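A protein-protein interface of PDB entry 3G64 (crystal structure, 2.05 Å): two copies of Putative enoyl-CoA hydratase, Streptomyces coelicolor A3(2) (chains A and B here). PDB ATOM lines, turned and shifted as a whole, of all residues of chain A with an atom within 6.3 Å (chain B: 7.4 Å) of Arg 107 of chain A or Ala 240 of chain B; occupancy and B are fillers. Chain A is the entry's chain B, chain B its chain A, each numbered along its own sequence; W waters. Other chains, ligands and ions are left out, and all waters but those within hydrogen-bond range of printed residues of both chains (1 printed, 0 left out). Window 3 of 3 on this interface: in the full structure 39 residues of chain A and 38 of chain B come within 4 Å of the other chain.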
ATOM      1  N   THR A 102     -22.190  -4.151 -15.801  1.00  0.00           N
ATOM      2  CA  THR A 102     -21.556  -2.876 -15.496  1.00  0.00           C
ATOM      3  C   THR A 102     -21.463  -2.666 -13.981  1.00  0.00           C
ATOM      4  O   THR A 102     -20.423  -2.239 -13.462  1.00  0.00           O
ATOM      5  CB  THR A 102     -22.288  -1.694 -16.173  1.00  0.00           C
ATOM      6  OG1 THR A 102     -23.665  -1.746 -15.818  1.00  0.00           O
ATOM      7  CG2 THR A 102     -22.148  -1.785 -17.719  1.00  0.00           C
ATOM      8  N   GLY A 103     -22.532  -2.993 -13.269  1.00  0.00           N
ATOM      9  CA  GLY A 103     -22.529  -2.862 -11.821  1.00  0.00           C
ATOM     10  C   GLY A 103     -21.511  -3.785 -11.164  1.00  0.00           C
ATOM     11  O   GLY A 103     -20.865  -3.397 -10.178  1.00  0.00           O
ATOM     12  N   GLN A 104     -21.371  -4.996 -11.708  1.00  0.00           N
ATOM     13  CA  GLN A 104     -20.365  -5.948 -11.229  1.00  0.00           C
ATOM     14  C   GLN A 104     -18.928  -5.441 -11.436  1.00  0.00           C
ATOM     15  O   GLN A 104     -18.039  -5.750 -10.643  1.00  0.00           O
ATOM     16  CB  GLN A 104     -20.487  -7.296 -11.942  1.00  0.00           C
ATOM     17  CG  GLN A 104     -21.585  -8.261 -11.488  1.00  0.00           C
ATOM     18  CD  GLN A 104     -21.618  -9.546 -12.377  1.00  0.00           C
ATOM     19  OE1 GLN A 104     -20.826  -9.696 -13.347  1.00  0.00           O
ATOM     20  NE2 GLN A 104     -22.534 -10.463 -12.056  1.00  0.00           N
ATOM     21  N   VAL A 105     -18.676  -4.691 -12.507  1.00  0.00           N
ATOM     22  CA  VAL A 105     -17.341  -4.118 -12.694  1.00  0.00           C
ATOM     23  C   VAL A 105     -17.046  -3.123 -11.559  1.00  0.00           C
ATOM     24  O   VAL A 105     -15.967  -3.131 -10.947  1.00  0.00           O
ATOM     25  CB  VAL A 105     -17.215  -3.432 -14.080  1.00  0.00           C
ATOM     26  CG1 VAL A 105     -15.948  -2.558 -14.170  1.00  0.00           C
ATOM     27  CG2 VAL A 105     -17.234  -4.504 -15.178  1.00  0.00           C
ATOM     28  N   VAL A 106     -18.016  -2.266 -11.280  1.00  0.00           N
ATOM     29  CA  VAL A 106     -17.885  -1.309 -10.180  1.00  0.00           C
ATOM     30  C   VAL A 106     -17.737  -2.041  -8.835  1.00  0.00           C
ATOM     31  O   VAL A 106     -16.870  -1.705  -8.030  1.00  0.00           O
ATOM     32  CB  VAL A 106     -19.068  -0.334 -10.138  1.00  0.00           C
ATOM     33  CG1 VAL A 106     -19.119   0.418  -8.787  1.00  0.00           C
ATOM     34  CG2 VAL A 106     -18.986   0.623 -11.317  1.00  0.00           C
ATOM     35  N   ARG A 107     -18.546  -3.060  -8.596  1.00  0.00           N
ATOM     36  CA  ARG A 107     -18.359  -3.825  -7.369  1.00  0.00           C
ATOM     37  C   ARG A 107     -16.968  -4.482  -7.262  1.00  0.00           C
ATOM     38  O   ARG A 107     -16.359  -4.523  -6.172  1.00  0.00           O
ATOM     39  CB  ARG A 107     -19.457  -4.864  -7.205  1.00  0.00           C
ATOM     40  CG  ARG A 107     -19.318  -5.599  -5.916  1.00  0.00           C
ATOM     41  CD  ARG A 107     -20.588  -6.318  -5.486  1.00  0.00           C
ATOM     42  NE  ARG A 107     -20.813  -7.540  -6.233  1.00  0.00           N
ATOM     43  CZ  ARG A 107     -21.241  -8.686  -5.694  1.00  0.00           C
ATOM     44  NH1 ARG A 107     -21.430  -9.734  -6.468  1.00  0.00           N
ATOM     45  NH2 ARG A 107     -21.452  -8.803  -4.385  1.00  0.00           N
ATOM     46  N   ALA A 108     -16.466  -4.996  -8.384  1.00  0.00           N
ATOM     47  CA  ALA A 108     -15.148  -5.637  -8.427  1.00  0.00           C
ATOM     48  C   ALA A 108     -14.035  -4.637  -8.119  1.00  0.00           C
ATOM     49  O   ALA A 108     -13.006  -4.992  -7.541  1.00  0.00           O
ATOM     50  CB  ALA A 108     -14.897  -6.282  -9.807  1.00  0.00           C
ATOM     51  N   VAL A 109     -14.221  -3.394  -8.544  1.00  0.00           N
ATOM     52  CA  VAL A 109     -13.259  -2.352  -8.209  1.00  0.00           C
ATOM     53  C   VAL A 109     -13.274  -2.097  -6.699  1.00  0.00           C
ATOM     54  O   VAL A 109     -12.221  -1.989  -6.082  1.00  0.00           O
ATOM     55  CB  VAL A 109     -13.515  -1.059  -8.998  1.00  0.00           C
ATOM     56  CG1 VAL A 109     -12.721   0.094  -8.414  1.00  0.00           C
ATOM     57  CG2 VAL A 109     -13.155  -1.265 -10.484  1.00  0.00           C
ATOM     58  N   ARG A 110     -14.461  -2.051  -6.100  1.00  0.00           N
ATOM     59  CA  ARG A 110     -14.569  -1.857  -4.655  1.00  0.00           C
ATOM     60  C   ARG A 110     -14.047  -3.047  -3.837  1.00  0.00           C
ATOM     61  O   ARG A 110     -13.685  -2.879  -2.660  1.00  0.00           O
ATOM     62  CB  ARG A 110     -16.021  -1.545  -4.234  1.00  0.00           C
ATOM     63  CG  ARG A 110     -16.617  -0.269  -4.900  1.00  0.00           C
ATOM     64  CD  ARG A 110     -15.858   1.040  -4.525  1.00  0.00           C
ATOM     65  NE  ARG A 110     -15.480   1.071  -3.109  1.00  0.00           N
ATOM     66  CZ  ARG A 110     -14.252   1.356  -2.670  1.00  0.00           C
ATOM     67  NH1 ARG A 110     -13.274   1.691  -3.527  1.00  0.00           N
ATOM     68  NH2 ARG A 110     -13.992   1.332  -1.372  1.00  0.00           N
ATOM     69  N   GLU A 111     -14.036  -4.235  -4.439  1.00  0.00           N
ATOM     70  CA  GLU A 111     -13.667  -5.468  -3.720  1.00  0.00           C
ATOM     71  C   GLU A 111     -12.274  -6.047  -4.006  1.00  0.00           C
ATOM     72  O   GLU A 111     -11.873  -7.032  -3.381  1.00  0.00           O
ATOM     73  CB  GLU A 111     -14.705  -6.578  -3.960  1.00  0.00           C
ATOM     74  CG  GLU A 111     -16.055  -6.287  -3.288  1.00  0.00           C
ATOM     75  CD  GLU A 111     -17.096  -7.388  -3.530  1.00  0.00           C
ATOM     76  OE1 GLU A 111     -18.145  -7.352  -2.850  1.00  0.00           O
ATOM     77  OE2 GLU A 111     -16.870  -8.280  -4.388  1.00  0.00           O
ATOM     78  N   CYS A 112     -11.544  -5.412  -4.919  1.00  0.00           N
ATOM     79  CA  CYS A 112     -10.159  -5.791  -5.218  1.00  0.00           C
ATOM     80  C   CYS A 112      -9.305  -5.783  -3.952  1.00  0.00           C
ATOM     81  O   CYS A 112      -9.405  -4.852  -3.153  1.00  0.00           O
ATOM     82  CB  CYS A 112      -9.553  -4.809  -6.225  1.00  0.00           C
ATOM     83  SG  CYS A 112     -10.103  -5.014  -7.933  1.00  0.00           S
ATOM     84  N   ALA A 134     -15.517   4.877  -8.239  1.00  0.00           N
ATOM     85  CA  ALA A 134     -15.277   3.604  -7.536  1.00  0.00           C
ATOM     86  C   ALA A 134     -13.828   3.385  -7.107  1.00  0.00           C
ATOM     87  O   ALA A 134     -13.545   2.595  -6.231  1.00  0.00           O
ATOM     88  CB  ALA A 134     -15.709   2.425  -8.436  1.00  0.00           C
ATOM     89  N   MET A 160     -24.989   1.601 -12.428  1.00  0.00           N
ATOM     90  CA  MET A 160     -23.801   0.842 -12.009  1.00  0.00           C
ATOM     91  C   MET A 160     -23.195   1.302 -10.667  1.00  0.00           C
ATOM     92  O   MET A 160     -21.979   1.344 -10.494  1.00  0.00           O
ATOM     93  CB  MET A 160     -22.737   0.787 -13.129  1.00  0.00           C
ATOM     94  CG  MET A 160     -22.233   2.120 -13.592  1.00  0.00           C
ATOM     95  SD  MET A 160     -21.278   2.082 -15.329  1.00  0.00           S
ATOM     96  CE  MET A 160     -19.619   1.219 -14.699  1.00  0.00           C
ATOM     97  N   TYR A 164     -25.388   4.708  -5.047  1.00  0.00           N
ATOM     98  CA  TYR A 164     -24.870   4.214  -3.784  1.00  0.00           C
ATOM     99  C   TYR A 164     -23.576   4.997  -3.467  1.00  0.00           C
ATOM    100  O   TYR A 164     -23.420   5.585  -2.387  1.00  0.00           O
ATOM    101  CB  TYR A 164     -24.634   2.680  -3.888  1.00  0.00           C
ATOM    102  CG  TYR A 164     -23.869   2.096  -2.729  1.00  0.00           C
ATOM    103  CD1 TYR A 164     -24.544   1.560  -1.609  1.00  0.00           C
ATOM    104  CD2 TYR A 164     -22.477   2.114  -2.716  1.00  0.00           C
ATOM    105  CE1 TYR A 164     -23.846   1.043  -0.526  1.00  0.00           C
ATOM    106  CE2 TYR A 164     -21.776   1.602  -1.633  1.00  0.00           C
ATOM    107  CZ  TYR A 164     -22.468   1.060  -0.542  1.00  0.00           C
ATOM    108  OH  TYR A 164     -21.759   0.560   0.544  1.00  0.00           O
ATOM    109  N   ASP A 236     -21.601  -0.739   5.094  1.00  0.00           N
ATOM    110  CA  ASP A 236     -22.858  -1.470   5.048  1.00  0.00           C
ATOM    111  C   ASP A 236     -23.156  -2.189   6.381  1.00  0.00           C
ATOM    112  O   ASP A 236     -23.998  -3.088   6.428  1.00  0.00           O
ATOM    113  CB  ASP A 236     -22.836  -2.506   3.905  1.00  0.00           C
ATOM    114  CG  ASP A 236     -22.724  -1.876   2.510  1.00  0.00           C
ATOM    115  OD1 ASP A 236     -23.112  -0.697   2.339  1.00  0.00           O
ATOM    116  OD2 ASP A 236     -22.265  -2.585   1.561  1.00  0.00           O
ATOM    117  N   MET B 237     -29.237   0.546   1.777  1.00  0.00           N
ATOM    118  CA  MET B 237     -28.900  -0.793   1.243  1.00  0.00           C
ATOM    119  C   MET B 237     -27.404  -1.011   1.165  1.00  0.00           C
ATOM    120  O   MET B 237     -26.658  -0.050   1.097  1.00  0.00           O
ATOM    121  CB  MET B 237     -29.436  -0.941  -0.186  1.00  0.00           C
ATOM    122  CG  MET B 237     -30.944  -0.839  -0.248  1.00  0.00           C
ATOM    123  SD  MET B 237     -31.569  -0.451  -2.091  1.00  0.00           S
ATOM    124  CE  MET B 237     -30.854  -2.049  -3.015  1.00  0.00           C
ATOM    125  N   PRO B 238     -26.971  -2.290   1.141  1.00  0.00           N
ATOM    126  CA  PRO B 238     -25.567  -2.631   0.918  1.00  0.00           C
ATOM    127  C   PRO B 238     -25.174  -2.556  -0.578  1.00  0.00           C
ATOM    128  O   PRO B 238     -26.022  -2.618  -1.474  1.00  0.00           O
ATOM    129  CB  PRO B 238     -25.485  -4.083   1.402  1.00  0.00           C
ATOM    130  CG  PRO B 238     -26.842  -4.633   1.093  1.00  0.00           C
ATOM    131  CD  PRO B 238     -27.770  -3.482   1.483  1.00  0.00           C
ATOM    132  N   LEU B 239     -23.874  -2.438  -0.831  1.00  0.00           N
ATOM    133  CA  LEU B 239     -23.368  -2.354  -2.205  1.00  0.00           C
ATOM    134  C   LEU B 239     -23.946  -3.436  -3.139  1.00  0.00           C
ATOM    135  O   LEU B 239     -24.463  -3.090  -4.213  1.00  0.00           O
ATOM    136  CB  LEU B 239     -21.840  -2.401  -2.212  1.00  0.00           C
ATOM    137  CG  LEU B 239     -21.146  -2.381  -3.584  1.00  0.00           C
ATOM    138  CD1 LEU B 239     -21.548  -1.134  -4.345  1.00  0.00           C
ATOM    139  CD2 LEU B 239     -19.634  -2.444  -3.393  1.00  0.00           C
ATOM    140  N   ALA B 240     -23.884  -4.728  -2.755  1.00  0.00           N
ATOM    141  CA  ALA B 240     -24.342  -5.791  -3.681  1.00  0.00           C
ATOM    142  C   ALA B 240     -25.815  -5.666  -4.051  1.00  0.00           C
ATOM    143  O   ALA B 240     -26.211  -5.950  -5.173  1.00  0.00           O
ATOM    144  CB  ALA B 240     -24.058  -7.198  -3.123  1.00  0.00           C
ATOM    145  N   ALA B 241     -26.637  -5.263  -3.092  1.00  0.00           N
ATOM    146  CA  ALA B 241     -28.057  -5.059  -3.370  1.00  0.00           C
ATOM    147  C   ALA B 241     -28.263  -3.808  -4.248  1.00  0.00           C
ATOM    148  O   ALA B 241     -29.141  -3.785  -5.115  1.00  0.00           O
ATOM    149  CB  ALA B 241     -28.840  -4.915  -2.048  1.00  0.00           C
ATOM    150  N   ALA B 242     -27.482  -2.751  -4.015  1.00  0.00           N
ATOM    151  CA  ALA B 242     -27.668  -1.531  -4.816  1.00  0.00           C
ATOM    152  C   ALA B 242     -27.442  -1.791  -6.320  1.00  0.00           C
ATOM    153  O   ALA B 242     -28.174  -1.281  -7.191  1.00  0.00           O
ATOM    154  CB  ALA B 242     -26.742  -0.408  -4.319  1.00  0.00           C
ATOM    155  N   VAL B 243     -26.449  -2.605  -6.647  1.00  0.00           N
ATOM    156  CA  VAL B 243     -26.206  -2.832  -8.064  1.00  0.00           C
ATOM    157  C   VAL B 243     -27.294  -3.724  -8.724  1.00  0.00           C
ATOM    158  O   VAL B 243     -27.536  -3.616  -9.930  1.00  0.00           O
ATOM    159  CB  VAL B 243     -24.730  -3.285  -8.354  1.00  0.00           C
ATOM    160  CG1 VAL B 243     -23.753  -2.138  -8.045  1.00  0.00           C
ATOM    161  CG2 VAL B 243     -24.373  -4.531  -7.580  1.00  0.00           C
ATOM    162  N   GLU B 244     -27.958  -4.574  -7.937  1.00  0.00           N
ATOM    163  CA  GLU B 244     -29.147  -5.306  -8.407  1.00  0.00           C
ATOM    164  C   GLU B 244     -30.337  -4.366  -8.711  1.00  0.00           C
ATOM    165  O   GLU B 244     -31.023  -4.511  -9.725  1.00  0.00           O
ATOM    166  CB  GLU B 244     -29.570  -6.362  -7.373  1.00  0.00           C
ATOM    167  CG  GLU B 244     -28.633  -7.540  -7.290  1.00  0.00           C
ATOM    168  CD  GLU B 244     -28.538  -8.272  -8.631  1.00  0.00           C
ATOM    169  OE1 GLU B 244     -29.601  -8.612  -9.185  1.00  0.00           O
ATOM    170  OE2 GLU B 244     -27.411  -8.466  -9.148  1.00  0.00           O
ATOM    171  N   LEU B 245     -30.583  -3.396  -7.833  1.00  0.00           N
ATOM    172  CA  LEU B 245     -31.643  -2.406  -8.078  1.00  0.00           C
ATOM    173  C   LEU B 245     -31.311  -1.546  -9.317  1.00  0.00           C
ATOM    174  O   LEU B 245     -32.172  -1.252 -10.138  1.00  0.00           O
ATOM    175  CB  LEU B 245     -31.845  -1.495  -6.848  1.00  0.00           C
ATOM    176  CG  LEU B 245     -32.892  -0.366  -6.904  1.00  0.00           C
ATOM    177  CD1 LEU B 245     -34.259  -0.901  -7.289  1.00  0.00           C
ATOM    178  CD2 LEU B 245     -32.991   0.423  -5.552  1.00  0.00           C
HETATM  179  O   HOH W   1     -25.168   0.991   3.095  1.00  0.00           O
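The side-chain carboxylate (OD2) of Asp 236 of chain A lies within hydrogen-bond range of the backbone NH (N) of Leu 239 of chain B (2.9 Å).
The side-chain carboxylate (OE1) of Glu 111 of chain A lies within salt-bridge range of the guanidinium group (NH2) of Arg 107 of chain A, 3.9 Å away.
NH1 of Arg 110 of chain A is in hydrogen-bond range of O of Ala 134 of chain A (2.9 Å).
OD1 of Asp 236 of chain A is in hydrogen-bond range of OH of Tyr 164 of chain A, 2.6 Å away.
Among the printed residues, pairs that only touch across the chains: Arg 107 of chain A with Ala 240 of chain B, Asp 236 of chain A with Pro 238 of chain B, Tyr 164 of chain A with Met 237 of chain B, Tyr 164 of chain A with Leu 239 of chain B, Tyr 164 of chain A with Ala 242 of chain B, Gly 103 of chain A with Val 243 of chain B, Asp 236 of chain A with Met 237 of chain B, Arg 110 of chain A with Leu 239 of chain B and Tyr 164 of chain A with Pro 238 of chain B.
Of the printed residues of chain B, Arg 107 of chain A touches Ala 240.
Of chain A, only Arg 107 (3.3 Å) comes within 4 Å of Ala 240 of chain B.
Of the printed residues of chain B, Asp 236 of chain A touches Met 237, Pro 238 and Leu 239.
Of the printed residues of chain A, Val 243 of chain B touches Gly 103.
Printed residues of chain B within 4 Å of Tyr 164 of chain A: Met 237 (3.4 Å), Pro 238 (3.8 Å), Leu 239 (3.5 Å) and Ala 242 (3.8 Å).
Printed residues of chain A within 4 Å of Leu 239 of chain B: Arg 110 (3.8 Å), Tyr 164 (3.5 Å) and Asp 236 (2.9 Å).
Printed residues of chain A that touch a printed residue of chain B: Gly 103, Arg 107, Arg 110, Tyr 164 and Asp 236.
Along chain B the printed residues that touch a printed residue of chain A span positions 237 to 243.
No position is printed for both chains.
Of the 10 pairs that touch across the chains among the printed residues, none has its exchanged pair printed and touching as well.
Water W1 lies within hydrogen-bond range of O of Met 237 of chain B (2.7 Å) and OD1 of Asp 236 of chain A (2.8 Å).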
